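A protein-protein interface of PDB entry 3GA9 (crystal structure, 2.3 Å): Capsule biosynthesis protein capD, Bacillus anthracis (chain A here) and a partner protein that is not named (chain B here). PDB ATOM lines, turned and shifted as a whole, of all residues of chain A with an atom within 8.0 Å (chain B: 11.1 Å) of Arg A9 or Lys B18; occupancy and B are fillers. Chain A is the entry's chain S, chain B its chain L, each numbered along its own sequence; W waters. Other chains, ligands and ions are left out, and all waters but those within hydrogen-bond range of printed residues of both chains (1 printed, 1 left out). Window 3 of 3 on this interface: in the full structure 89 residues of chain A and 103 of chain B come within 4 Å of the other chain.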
ATOM      1  N   ILE A   6      29.543  21.981   2.851  1.00  0.00           N
ATOM      2  CA  ILE A   6      28.497  21.116   3.356  1.00  0.00           C
ATOM      3  C   ILE A   6      27.892  21.749   4.603  1.00  0.00           C
ATOM      4  O   ILE A   6      28.609  22.266   5.459  1.00  0.00           O
ATOM      5  CB  ILE A   6      29.047  19.742   3.763  1.00  0.00           C
ATOM      6  CG1 ILE A   6      29.767  19.104   2.564  1.00  0.00           C
ATOM      7  CG2 ILE A   6      27.896  18.899   4.340  1.00  0.00           C
ATOM      8  CD1 ILE A   6      30.188  17.670   2.727  1.00  0.00           C
ATOM      9  N   ILE A   7      26.575  21.694   4.710  1.00  0.00           N
ATOM     10  CA  ILE A   7      25.899  22.114   5.936  1.00  0.00           C
ATOM     11  C   ILE A   7      24.980  20.980   6.384  1.00  0.00           C
ATOM     12  O   ILE A   7      24.146  20.559   5.582  1.00  0.00           O
ATOM     13  CB  ILE A   7      25.105  23.418   5.692  1.00  0.00           C
ATOM     14  CG1 ILE A   7      26.066  24.571   5.416  1.00  0.00           C
ATOM     15  CG2 ILE A   7      24.204  23.714   6.896  1.00  0.00           C
ATOM     16  CD1 ILE A   7      25.406  25.952   5.082  1.00  0.00           C
ATOM     17  N   ASP A   8      25.141  20.475   7.627  1.00  0.00           N
ATOM     18  CA  ASP A   8      24.274  19.381   8.133  1.00  0.00           C
ATOM     19  C   ASP A   8      23.093  19.817   9.038  1.00  0.00           C
ATOM     20  O   ASP A   8      22.944  21.009   9.356  1.00  0.00           O
ATOM     21  CB  ASP A   8      25.079  18.265   8.817  1.00  0.00           C
ATOM     22  CG  ASP A   8      25.646  18.685  10.169  1.00  0.00           C
ATOM     23  OD1 ASP A   8      25.249  19.758  10.689  1.00  0.00           O
ATOM     24  OD2 ASP A   8      26.499  17.951  10.725  1.00  0.00           O
ATOM     25  N   ARG A   9      22.293  18.829   9.455  1.00  0.00           N
ATOM     26  CA  ARG A   9      21.119  19.036  10.312  1.00  0.00           C
ATOM     27  C   ARG A   9      21.277  19.993  11.468  1.00  0.00           C
ATOM     28  O   ARG A   9      20.404  20.809  11.682  1.00  0.00           O
ATOM     29  CB  ARG A   9      20.569  17.725  10.840  1.00  0.00           C
ATOM     30  CG  ARG A   9      19.505  17.209   9.938  1.00  0.00           C
ATOM     31  CD  ARG A   9      19.036  15.842  10.325  1.00  0.00           C
ATOM     32  NE  ARG A   9      18.216  15.315   9.231  1.00  0.00           N
ATOM     33  CZ  ARG A   9      18.679  14.553   8.237  1.00  0.00           C
ATOM     34  NH1 ARG A   9      19.959  14.198   8.197  1.00  0.00           N
ATOM     35  NH2 ARG A   9      17.845  14.128   7.296  1.00  0.00           N
ATOM     36  N   ASP A  10      22.353  19.898  12.231  1.00  0.00           N
ATOM     37  CA  ASP A  10      22.491  20.846  13.333  1.00  0.00           C
ATOM     38  C   ASP A  10      23.386  22.045  13.018  1.00  0.00           C
ATOM     39  O   ASP A  10      24.036  22.597  13.899  1.00  0.00           O
ATOM     40  CB  ASP A  10      22.846  20.156  14.656  1.00  0.00           C
ATOM     41  CG  ASP A  10      23.782  19.010  14.466  1.00  0.00           C
ATOM     42  OD1 ASP A  10      24.876  19.253  13.912  1.00  0.00           O
ATOM     43  OD2 ASP A  10      23.428  17.876  14.854  1.00  0.00           O
ATOM     44  N   GLY A  11      23.367  22.445  11.743  1.00  0.00           N
ATOM     45  CA  GLY A  11      24.021  23.654  11.279  1.00  0.00           C
ATOM     46  C   GLY A  11      25.536  23.686  11.339  1.00  0.00           C
ATOM     47  O   GLY A  11      26.129  24.759  11.320  1.00  0.00           O
ATOM     48  N   THR A  12      26.173  22.529  11.445  1.00  0.00           N
ATOM     49  CA  THR A  12      27.607  22.475  11.206  1.00  0.00           C
ATOM     50  C   THR A  12      27.876  22.709   9.728  1.00  0.00           C
ATOM     51  O   THR A  12      27.231  22.113   8.863  1.00  0.00           O
ATOM     52  CB  THR A  12      28.204  21.142  11.629  1.00  0.00           C
ATOM     53  OG1 THR A  12      28.036  21.006  13.042  1.00  0.00           O
ATOM     54  CG2 THR A  12      29.706  21.098  11.303  1.00  0.00           C
ATOM     55  N   LYS A 154      22.702  28.769   4.858  1.00  0.00           N
ATOM     56  CA  LYS A 154      21.566  28.431   5.694  1.00  0.00           C
ATOM     57  C   LYS A 154      21.002  29.695   6.315  1.00  0.00           C
ATOM     58  O   LYS A 154      21.731  30.451   6.949  1.00  0.00           O
ATOM     59  CB  LYS A 154      21.954  27.490   6.815  1.00  0.00           C
ATOM     60  CG  LYS A 154      20.794  27.180   7.753  1.00  0.00           C
ATOM     61  CD  LYS A 154      21.240  26.314   8.925  1.00  0.00           C
ATOM     62  CE  LYS A 154      20.058  25.985   9.831  1.00  0.00           C
ATOM     63  NZ  LYS A 154      20.461  25.291  11.097  1.00  0.00           N
ATOM     64  N   ASN A 159      14.331  26.068   8.431  1.00  0.00           N
ATOM     65  CA  ASN A 159      15.443  26.699   7.735  1.00  0.00           C
ATOM     66  C   ASN A 159      15.368  26.373   6.258  1.00  0.00           C
ATOM     67  O   ASN A 159      14.713  25.414   5.840  1.00  0.00           O
ATOM     68  CB  ASN A 159      16.758  26.197   8.316  1.00  0.00           C
ATOM     69  CG  ASN A 159      16.668  25.968   9.808  1.00  0.00           C
ATOM     70  OD1 ASN A 159      16.338  26.889  10.564  1.00  0.00           O
ATOM     71  ND2 ASN A 159      16.938  24.731  10.245  1.00  0.00           N
ATOM     72  N   ILE A 161      18.116  26.024   3.093  1.00  0.00           N
ATOM     73  CA  ILE A 161      19.471  26.087   2.601  1.00  0.00           C
ATOM     74  C   ILE A 161      19.383  26.399   1.142  1.00  0.00           C
ATOM     75  O   ILE A 161      18.546  25.866   0.418  1.00  0.00           O
ATOM     76  CB  ILE A 161      20.292  24.809   2.910  1.00  0.00           C
ATOM     77  CG1 ILE A 161      20.845  24.902   4.329  1.00  0.00           C
ATOM     78  CG2 ILE A 161      21.465  24.685   1.964  1.00  0.00           C
ATOM     79  CD1 ILE A 161      21.003  23.599   5.008  1.00  0.00           C
ATOM     80  N   ASN A 176      17.859  19.591   1.041  1.00  0.00           N
ATOM     81  CA  ASN A 176      16.690  18.704   1.167  1.00  0.00           C
ATOM     82  C   ASN A 176      15.315  19.351   0.922  1.00  0.00           C
ATOM     83  O   ASN A 176      15.168  20.588   1.006  1.00  0.00           O
ATOM     84  CB  ASN A 176      16.690  18.020   2.521  1.00  0.00           C
ATOM     85  CG  ASN A 176      16.471  18.982   3.661  1.00  0.00           C
ATOM     86  OD1 ASN A 176      16.822  20.170   3.585  1.00  0.00           O
ATOM     87  ND2 ASN A 176      15.890  18.471   4.743  1.00  0.00           N
ATOM     88  N   LYS B  18      15.339  15.549  10.295  1.00  0.00           N
ATOM     89  CA  LYS B  18      14.660  16.501   9.339  1.00  0.00           C
ATOM     90  C   LYS B  18      14.133  17.819   9.990  1.00  0.00           C
ATOM     91  O   LYS B  18      12.944  17.919  10.347  1.00  0.00           O
ATOM     92  CB  LYS B  18      13.569  15.781   8.499  1.00  0.00           C
ATOM     93  CG  LYS B  18      13.154  14.405   9.027  1.00  0.00           C
ATOM     94  CD  LYS B  18      11.809  14.512   9.816  1.00  0.00           C
ATOM     95  CE  LYS B  18      11.623  13.212  10.617  1.00  0.00           C
ATOM     96  NZ  LYS B  18      10.208  13.054  11.058  1.00  0.00           N
ATOM     97  N   GLY B  19      15.005  18.829  10.145  1.00  0.00           N
ATOM     98  CA  GLY B  19      16.404  18.754   9.746  1.00  0.00           C
ATOM     99  C   GLY B  19      16.598  19.272   8.328  1.00  0.00           C
ATOM    100  O   GLY B  19      16.074  18.716   7.355  1.00  0.00           O
ATOM    101  N   THR B  20      17.352  20.350   8.206  1.00  0.00           N
ATOM    102  CA  THR B  20      17.679  20.896   6.900  1.00  0.00           C
ATOM    103  C   THR B  20      19.174  20.596   6.633  1.00  0.00           C
ATOM    104  O   THR B  20      19.959  20.513   7.591  1.00  0.00           O
ATOM    105  CB  THR B  20      17.365  22.398   6.896  1.00  0.00           C
ATOM    106  OG1 THR B  20      17.732  22.973   5.641  1.00  0.00           O
ATOM    107  CG2 THR B  20      18.144  23.092   7.967  1.00  0.00           C
ATOM    108  N   TYR B  21      19.558  20.415   5.359  1.00  0.00           N
ATOM    109  CA  TYR B  21      20.960  20.080   4.983  1.00  0.00           C
ATOM    110  C   TYR B  21      21.259  20.239   3.467  1.00  0.00           C
ATOM    111  O   TYR B  21      20.344  20.189   2.617  1.00  0.00           O
ATOM    112  CB  TYR B  21      21.362  18.661   5.469  1.00  0.00           C
ATOM    113  CG  TYR B  21      20.482  17.591   4.865  1.00  0.00           C
ATOM    114  CD1 TYR B  21      19.452  16.995   5.608  1.00  0.00           C
ATOM    115  CD2 TYR B  21      20.626  17.225   3.517  1.00  0.00           C
ATOM    116  CE1 TYR B  21      18.605  16.034   5.021  1.00  0.00           C
ATOM    117  CE2 TYR B  21      19.802  16.291   2.927  1.00  0.00           C
ATOM    118  CZ  TYR B  21      18.796  15.691   3.676  1.00  0.00           C
ATOM    119  OH  TYR B  21      17.985  14.766   3.069  1.00  0.00           O
ATOM    120  N   GLY B  22      22.539  20.414   3.129  1.00  0.00           N
ATOM    121  CA  GLY B  22      22.916  20.606   1.732  1.00  0.00           C
ATOM    122  C   GLY B  22      24.364  20.336   1.380  1.00  0.00           C
ATOM    123  O   GLY B  22      25.208  20.268   2.238  1.00  0.00           O
ATOM    124  N   VAL B  23      24.642  20.194   0.095  1.00  0.00           N
ATOM    125  CA  VAL B  23      26.002  20.040  -0.416  1.00  0.00           C
ATOM    126  C   VAL B  23      26.252  20.974  -1.636  1.00  0.00           C
ATOM    127  O   VAL B  23      25.428  21.023  -2.563  1.00  0.00           O
ATOM    128  CB  VAL B  23      26.259  18.594  -0.912  1.00  0.00           C
ATOM    129  CG1 VAL B  23      27.711  18.456  -1.411  1.00  0.00           C
ATOM    130  CG2 VAL B  23      25.923  17.519   0.183  1.00  0.00           C
ATOM    131  N   GLY B  34      27.243  13.164  -1.327  1.00  0.00           N
ATOM    132  CA  GLY B  34      27.152  13.971  -0.147  1.00  0.00           C
ATOM    133  C   GLY B  34      25.744  13.993   0.415  1.00  0.00           C
ATOM    134  O   GLY B  34      25.545  13.758   1.610  1.00  0.00           O
ATOM    135  N   MET B  35      24.783  14.281  -0.456  1.00  0.00           N
ATOM    136  CA  MET B  35      23.383  14.324  -0.062  1.00  0.00           C
ATOM    137  C   MET B  35      22.948  12.951   0.489  1.00  0.00           C
ATOM    138  O   MET B  35      22.188  12.906   1.445  1.00  0.00           O
ATOM    139  CB  MET B  35      22.486  14.764  -1.240  1.00  0.00           C
ATOM    140  CG  MET B  35      22.670  16.211  -1.647  1.00  0.00           C
ATOM    141  SD  MET B  35      22.044  17.310  -0.224  1.00  0.00           S
ATOM    142  CE  MET B  35      20.143  16.959  -0.575  1.00  0.00           C
ATOM    143  N   LYS B  36      23.469  11.855  -0.080  1.00  0.00           N
ATOM    144  CA  LYS B  36      23.129  10.488   0.360  1.00  0.00           C
ATOM    145  C   LYS B  36      23.440  10.272   1.833  1.00  0.00           C
ATOM    146  O   LYS B  36      22.600   9.800   2.592  1.00  0.00           O
ATOM    147  CB  LYS B  36      23.884   9.469  -0.472  1.00  0.00           C
ATOM    148  CG  LYS B  36      23.161   8.131  -0.695  1.00  0.00           C
ATOM    149  CD  LYS B  36      23.264   7.728  -2.177  1.00  0.00           C
ATOM    150  CE  LYS B  36      23.407   6.227  -2.364  1.00  0.00           C
ATOM    151  NZ  LYS B  36      24.367   5.668  -1.359  1.00  0.00           N
ATOM    152  N   VAL B  37      24.653  10.638   2.229  1.00  0.00           N
ATOM    153  CA  VAL B  37      25.104  10.562   3.612  1.00  0.00           C
ATOM    154  C   VAL B  37      24.251  11.450   4.500  1.00  0.00           C
ATOM    155  O   VAL B  37      23.908  11.089   5.623  1.00  0.00           O
ATOM    156  CB  VAL B  37      26.558  11.069   3.702  1.00  0.00           C
ATOM    157  CG1 VAL B  37      27.091  10.978   5.109  1.00  0.00           C
ATOM    158  CG2 VAL B  37      27.443  10.294   2.739  1.00  0.00           C
ATOM    159  N   LEU B  38      23.944  12.641   4.006  1.00  0.00           N
ATOM    160  CA  LEU B  38      23.184  13.583   4.782  1.00  0.00           C
ATOM    161  C   LEU B  38      21.726  13.107   4.953  1.00  0.00           C
ATOM    162  O   LEU B  38      21.232  13.102   6.055  1.00  0.00           O
ATOM    163  CB  LEU B  38      23.261  14.969   4.165  1.00  0.00           C
ATOM    164  CG  LEU B  38      24.618  15.687   4.190  1.00  0.00           C
ATOM    165  CD1 LEU B  38      24.525  16.992   3.392  1.00  0.00           C
ATOM    166  CD2 LEU B  38      25.127  15.928   5.596  1.00  0.00           C
ATOM    167  N   LYS B  39      21.080  12.707   3.858  1.00  0.00           N
ATOM    168  CA  LYS B  39      19.741  12.088   3.846  1.00  0.00           C
ATOM    169  C   LYS B  39      19.547  11.019   4.909  1.00  0.00           C
ATOM    170  O   LYS B  39      18.512  10.988   5.567  1.00  0.00           O
ATOM    171  CB  LYS B  39      19.453  11.497   2.462  1.00  0.00           C
ATOM    172  CG  LYS B  39      18.130  10.715   2.290  1.00  0.00           C
ATOM    173  CD  LYS B  39      18.055  10.123   0.839  1.00  0.00           C
ATOM    174  CE  LYS B  39      16.932   9.070   0.628  1.00  0.00           C
ATOM    175  NZ  LYS B  39      15.535   9.644   0.708  1.00  0.00           N
ATOM    176  N   ASN B  40      20.543  10.165   5.086  1.00  0.00           N
ATOM    177  CA  ASN B  40      20.471   9.086   6.047  1.00  0.00           C
ATOM    178  C   ASN B  40      20.955   9.482   7.433  1.00  0.00           C
ATOM    179  O   ASN B  40      21.240   8.625   8.271  1.00  0.00           O
ATOM    180  CB  ASN B  40      21.264   7.900   5.537  1.00  0.00           C
ATOM    181  CG  ASN B  40      20.727   7.385   4.250  1.00  0.00           C
ATOM    182  OD1 ASN B  40      21.481   7.055   3.349  1.00  0.00           O
ATOM    183  ND2 ASN B  40      19.408   7.333   4.132  1.00  0.00           N
ATOM    184  N   GLY B  41      21.070  10.786   7.656  1.00  0.00           N
ATOM    185  CA  GLY B  41      21.355  11.309   8.972  1.00  0.00           C
ATOM    186  C   GLY B  41      22.796  11.527   9.343  1.00  0.00           C
ATOM    187  O   GLY B  41      23.083  11.732  10.512  1.00  0.00           O
ATOM    188  N   GLY B  42      23.714  11.496   8.387  1.00  0.00           N
ATOM    189  CA  GLY B  42      25.113  11.748   8.712  1.00  0.00           C
ATOM    190  C   GLY B  42      25.502  13.211   8.974  1.00  0.00           C
ATOM    191  O   GLY B  42      24.779  14.158   8.613  1.00  0.00           O
ATOM    192  N   SER B  43      26.668  13.383   9.593  1.00  0.00           N
ATOM    193  CA  SER B  43      27.216  14.681   9.927  1.00  0.00           C
ATOM    194  C   SER B  43      27.915  15.317   8.712  1.00  0.00           C
ATOM    195  O   SER B  43      28.192  14.643   7.714  1.00  0.00           O
ATOM    196  CB  SER B  43      28.229  14.518  11.053  1.00  0.00           C
ATOM    197  OG  SER B  43      29.337  13.739  10.608  1.00  0.00           O
ATOM    198  N   ALA B  44      28.226  16.609   8.832  1.00  0.00           N
ATOM    199  CA  ALA B  44      28.819  17.368   7.741  1.00  0.00           C
ATOM    200  C   ALA B  44      30.224  16.870   7.460  1.00  0.00           C
ATOM    201  O   ALA B  44      30.651  16.878   6.307  1.00  0.00           O
ATOM    202  CB  ALA B  44      28.810  18.871   8.027  1.00  0.00           C
ATOM    203  N   VAL B  45      30.924  16.395   8.490  1.00  0.00           N
ATOM    204  CA  VAL B  45      32.286  15.879   8.283  1.00  0.00           C
ATOM    205  C   VAL B  45      32.342  14.463   7.684  1.00  0.00           C
ATOM    206  O   VAL B  45      33.245  14.152   6.896  1.00  0.00           O
ATOM    207  CB  VAL B  45      33.180  15.986   9.550  1.00  0.00           C
ATOM    208  CG1 VAL B  45      33.022  17.370  10.183  1.00  0.00           C
ATOM    209  CG2 VAL B  45      32.883  14.886  10.524  1.00  0.00           C
ATOM    210  N   ASP B  46      31.389  13.610   8.051  1.00  0.00           N
ATOM    211  CA  ASP B  46      31.260  12.324   7.372  1.00  0.00           C
ATOM    212  C   ASP B  46      30.925  12.555   5.892  1.00  0.00           C
ATOM    213  O   ASP B  46      31.526  11.933   5.010  1.00  0.00           O
ATOM    214  CB  ASP B  46      30.214  11.423   8.049  1.00  0.00           C
ATOM    215  CG  ASP B  46      30.661  10.941   9.460  1.00  0.00           C
ATOM    216  OD1 ASP B  46      31.859  11.072   9.834  1.00  0.00           O
ATOM    217  OD2 ASP B  46      29.801  10.406  10.207  1.00  0.00           O
ATOM    218  N   ALA B  47      29.978  13.453   5.618  1.00  0.00           N
ATOM    219  CA  ALA B  47      29.658  13.812   4.221  1.00  0.00           C
ATOM    220  C   ALA B  47      30.894  14.384   3.492  1.00  0.00           C
ATOM    221  O   ALA B  47      31.095  14.071   2.329  1.00  0.00           O
ATOM    222  CB  ALA B  47      28.501  14.788   4.158  1.00  0.00           C
ATOM    223  N   ILE B  74      33.203  24.590  11.114  1.00  0.00           N
ATOM    224  CA  ILE B  74      32.517  25.458  12.078  1.00  0.00           C
ATOM    225  C   ILE B  74      31.175  24.848  12.510  1.00  0.00           C
ATOM    226  O   ILE B  74      30.258  24.680  11.682  1.00  0.00           O
ATOM    227  CB  ILE B  74      32.235  26.861  11.507  1.00  0.00           C
ATOM    228  CG1 ILE B  74      33.461  27.451  10.792  1.00  0.00           C
ATOM    229  CG2 ILE B  74      31.673  27.788  12.626  1.00  0.00           C
ATOM    230  CD1 ILE B  74      34.748  27.497  11.592  1.00  0.00           C
ATOM    231  N   SER B  75      31.091  24.506  13.801  1.00  0.00           N
ATOM    232  CA  SER B  75      29.847  24.052  14.436  1.00  0.00           C
ATOM    233  C   SER B  75      29.395  25.058  15.513  1.00  0.00           C
ATOM    234  O   SER B  75      30.109  26.041  15.784  1.00  0.00           O
ATOM    235  CB  SER B  75      30.043  22.665  15.059  1.00  0.00           C
ATOM    236  OG  SER B  75      31.116  22.691  15.986  1.00  0.00           O
ATOM    237  N   LYS B  76      28.208  24.816  16.055  1.00  0.00           N
ATOM    238  CA  LYS B  76      27.561  25.730  16.980  1.00  0.00           C
ATOM    239  C   LYS B  76      28.512  26.254  18.006  1.00  0.00           C
ATOM    240  O   LYS B  76      28.572  27.445  18.215  1.00  0.00           O
ATOM    241  CB  LYS B  76      26.363  25.094  17.640  1.00  0.00           C
ATOM    242  CG  LYS B  76      25.071  25.540  17.030  1.00  0.00           C
ATOM    243  CD  LYS B  76      24.238  24.373  16.540  1.00  0.00           C
ATOM    244  CE  LYS B  76      22.768  24.756  16.323  1.00  0.00           C
ATOM    245  NZ  LYS B  76      21.969  23.760  15.544  1.00  0.00           N
ATOM    246  N   LEU B 118      30.451   7.978  11.486  1.00  0.00           N
ATOM    247  CA  LEU B 118      30.331   6.767  10.662  1.00  0.00           C
ATOM    248  C   LEU B 118      31.663   6.015  10.509  1.00  0.00           C
ATOM    249  O   LEU B 118      32.744   6.621  10.679  1.00  0.00           O
ATOM    250  CB  LEU B 118      29.711   7.113   9.320  1.00  0.00           C
ATOM    251  CG  LEU B 118      28.225   7.444   9.406  1.00  0.00           C
ATOM    252  CD1 LEU B 118      27.823   8.282   8.186  1.00  0.00           C
ATOM    253  CD2 LEU B 118      27.392   6.159   9.468  1.00  0.00           C
HETATM  254  O   HOH W   1      26.617  22.564  14.888  1.00  0.00           O
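ND2 of Asn A176 is in hydrogen-bond range of O of Gly B19, 2.6 Å away. O of Thr B20 sits close to N of Arg A9 (3.4 Å). The backbone NH of Asn A176 lies within hydrogen-bond range of the backbone carbonyl oxygen of Tyr B21, at 3.0 Å. The backbone carbonyl oxygen of Ile A7 is in hydrogen-bond range of the backbone NH of Gly B22, at 2.9 Å. O of Leu B38 lies within hydrogen-bond range of NH1 of Arg A9, 2.7 Å away. N of Ala B44 sits at hydrogen-bond distance from OD2 of Asp A8 (2.9 Å). NZ of Lys B76 sits at hydrogen-bond distance from O of Asp A10, at 2.9 Å. NE of Arg A9 sits close to N of Lys B18.
The backbone NH (N) of Asp B46 sits at hydrogen-bond distance from the side-chain hydroxyl (OG) of Ser B43, at 3.3 Å. The backbone NH (N) of Asp A10 lies close to the side-chain carboxylate (OD1) of Asp A8, 3.3 Å away. OD1 of Asp A8 lies within hydrogen-bond range of N of Gly A11. OD1 of Asp A8 sits at hydrogen-bond distance from N of Thr A12 (3.0 Å).
Among the printed residues, merely in contact across the chains: Ile A6 with Gly B22 (3.6 Å), Ile A6 with Leu B38 (3.99 Å), Ile A6 with Ala B44 (3.7 Å), Ile A6 with Ala B47 (3.4 Å), Ile A7 with Tyr B21 (3.3 Å), Asp A8 with Thr B20 (3.5 Å), Asp A8 with Leu B38 (3.98 Å), Asp A8 with Ser B43 (3.4 Å), Arg A9 with Gly B19 (3.5 Å), Arg A9 with Tyr B21 (3.1 Å), Arg A9 with Lys B39 (3.6 Å), Arg A9 with Gly B41 (3.3 Å), Thr A12 with Ala B44 (3.7 Å), Thr A12 with Ile B74 (3.5 Å), Thr A12 with Ser B75 (3.3 Å), Lys A154 with Thr B20 (3.9 Å), Asn A159 with Thr B20 (3.1 Å), Ile A161 with Thr B20 (3.4 Å), Ile A161 with Tyr B21 (3.5 Å), Asn A176 with Thr B20 (3.5 Å) and Asn A176 with Met B35 (3.8 Å).
Arg A9 touches just these residues of chain B: Lys B18, Gly B19, Thr B20, Tyr B21, Leu B38, Lys B39 and Gly B41. No residue of chain B comes within 4 Å of Gly A11. Printed residues of chain A within 4 Å of Ser B75: Thr A12. Of the printed residues of chain A, Leu B38 touches Ile A6, Asp A8 and Arg A9. Printed residues of chain A within 4 Å of Gly B41: Arg A9. Printed residues of chain B within 4 Å of Asn A176: Gly B19, Thr B20, Tyr B21 and Met B35. Val B23 touches none of the printed residues of chain A. The nearest residue of chain B that does not touch Arg A9 is Gly B42 (4.6 Å). The nearest printed residue of chain A that does not touch Lys B39 is Asn A176 (6.8 Å).
Hydrophobic or aromatic side chains of chain A within 4 Å of the printed part of chain B: Ile A6 and Ile A161. Printed residues of chain B that touch a printed residue of chain A: Lys B18, Gly B19, Thr B20, Tyr B21, Gly B22, Met B35, Leu B38, Lys B39, Gly B41, Ser B43, Ala B44, Ala B47, Ile B74, Ser B75 and Lys B76. Hydrophobic or aromatic side chains of chain B that line the printed part of chain A: Tyr B21, Met B35, Leu B38, Ala B44 and Ala B47. Among the printed residues, 29 pairs touch across the chains. Among the printed residues, no Asp or Glu carboxylate lies within 4 Å of a Lys or Arg side-chain nitrogen of the other chain.
Water W1 lies within hydrogen-bond range of the backbone carbonyl oxygen (O) of Asp A10, the side-chain hydroxyl (OG1) of Thr A12 and the backbone NH (N) of Lys B76.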
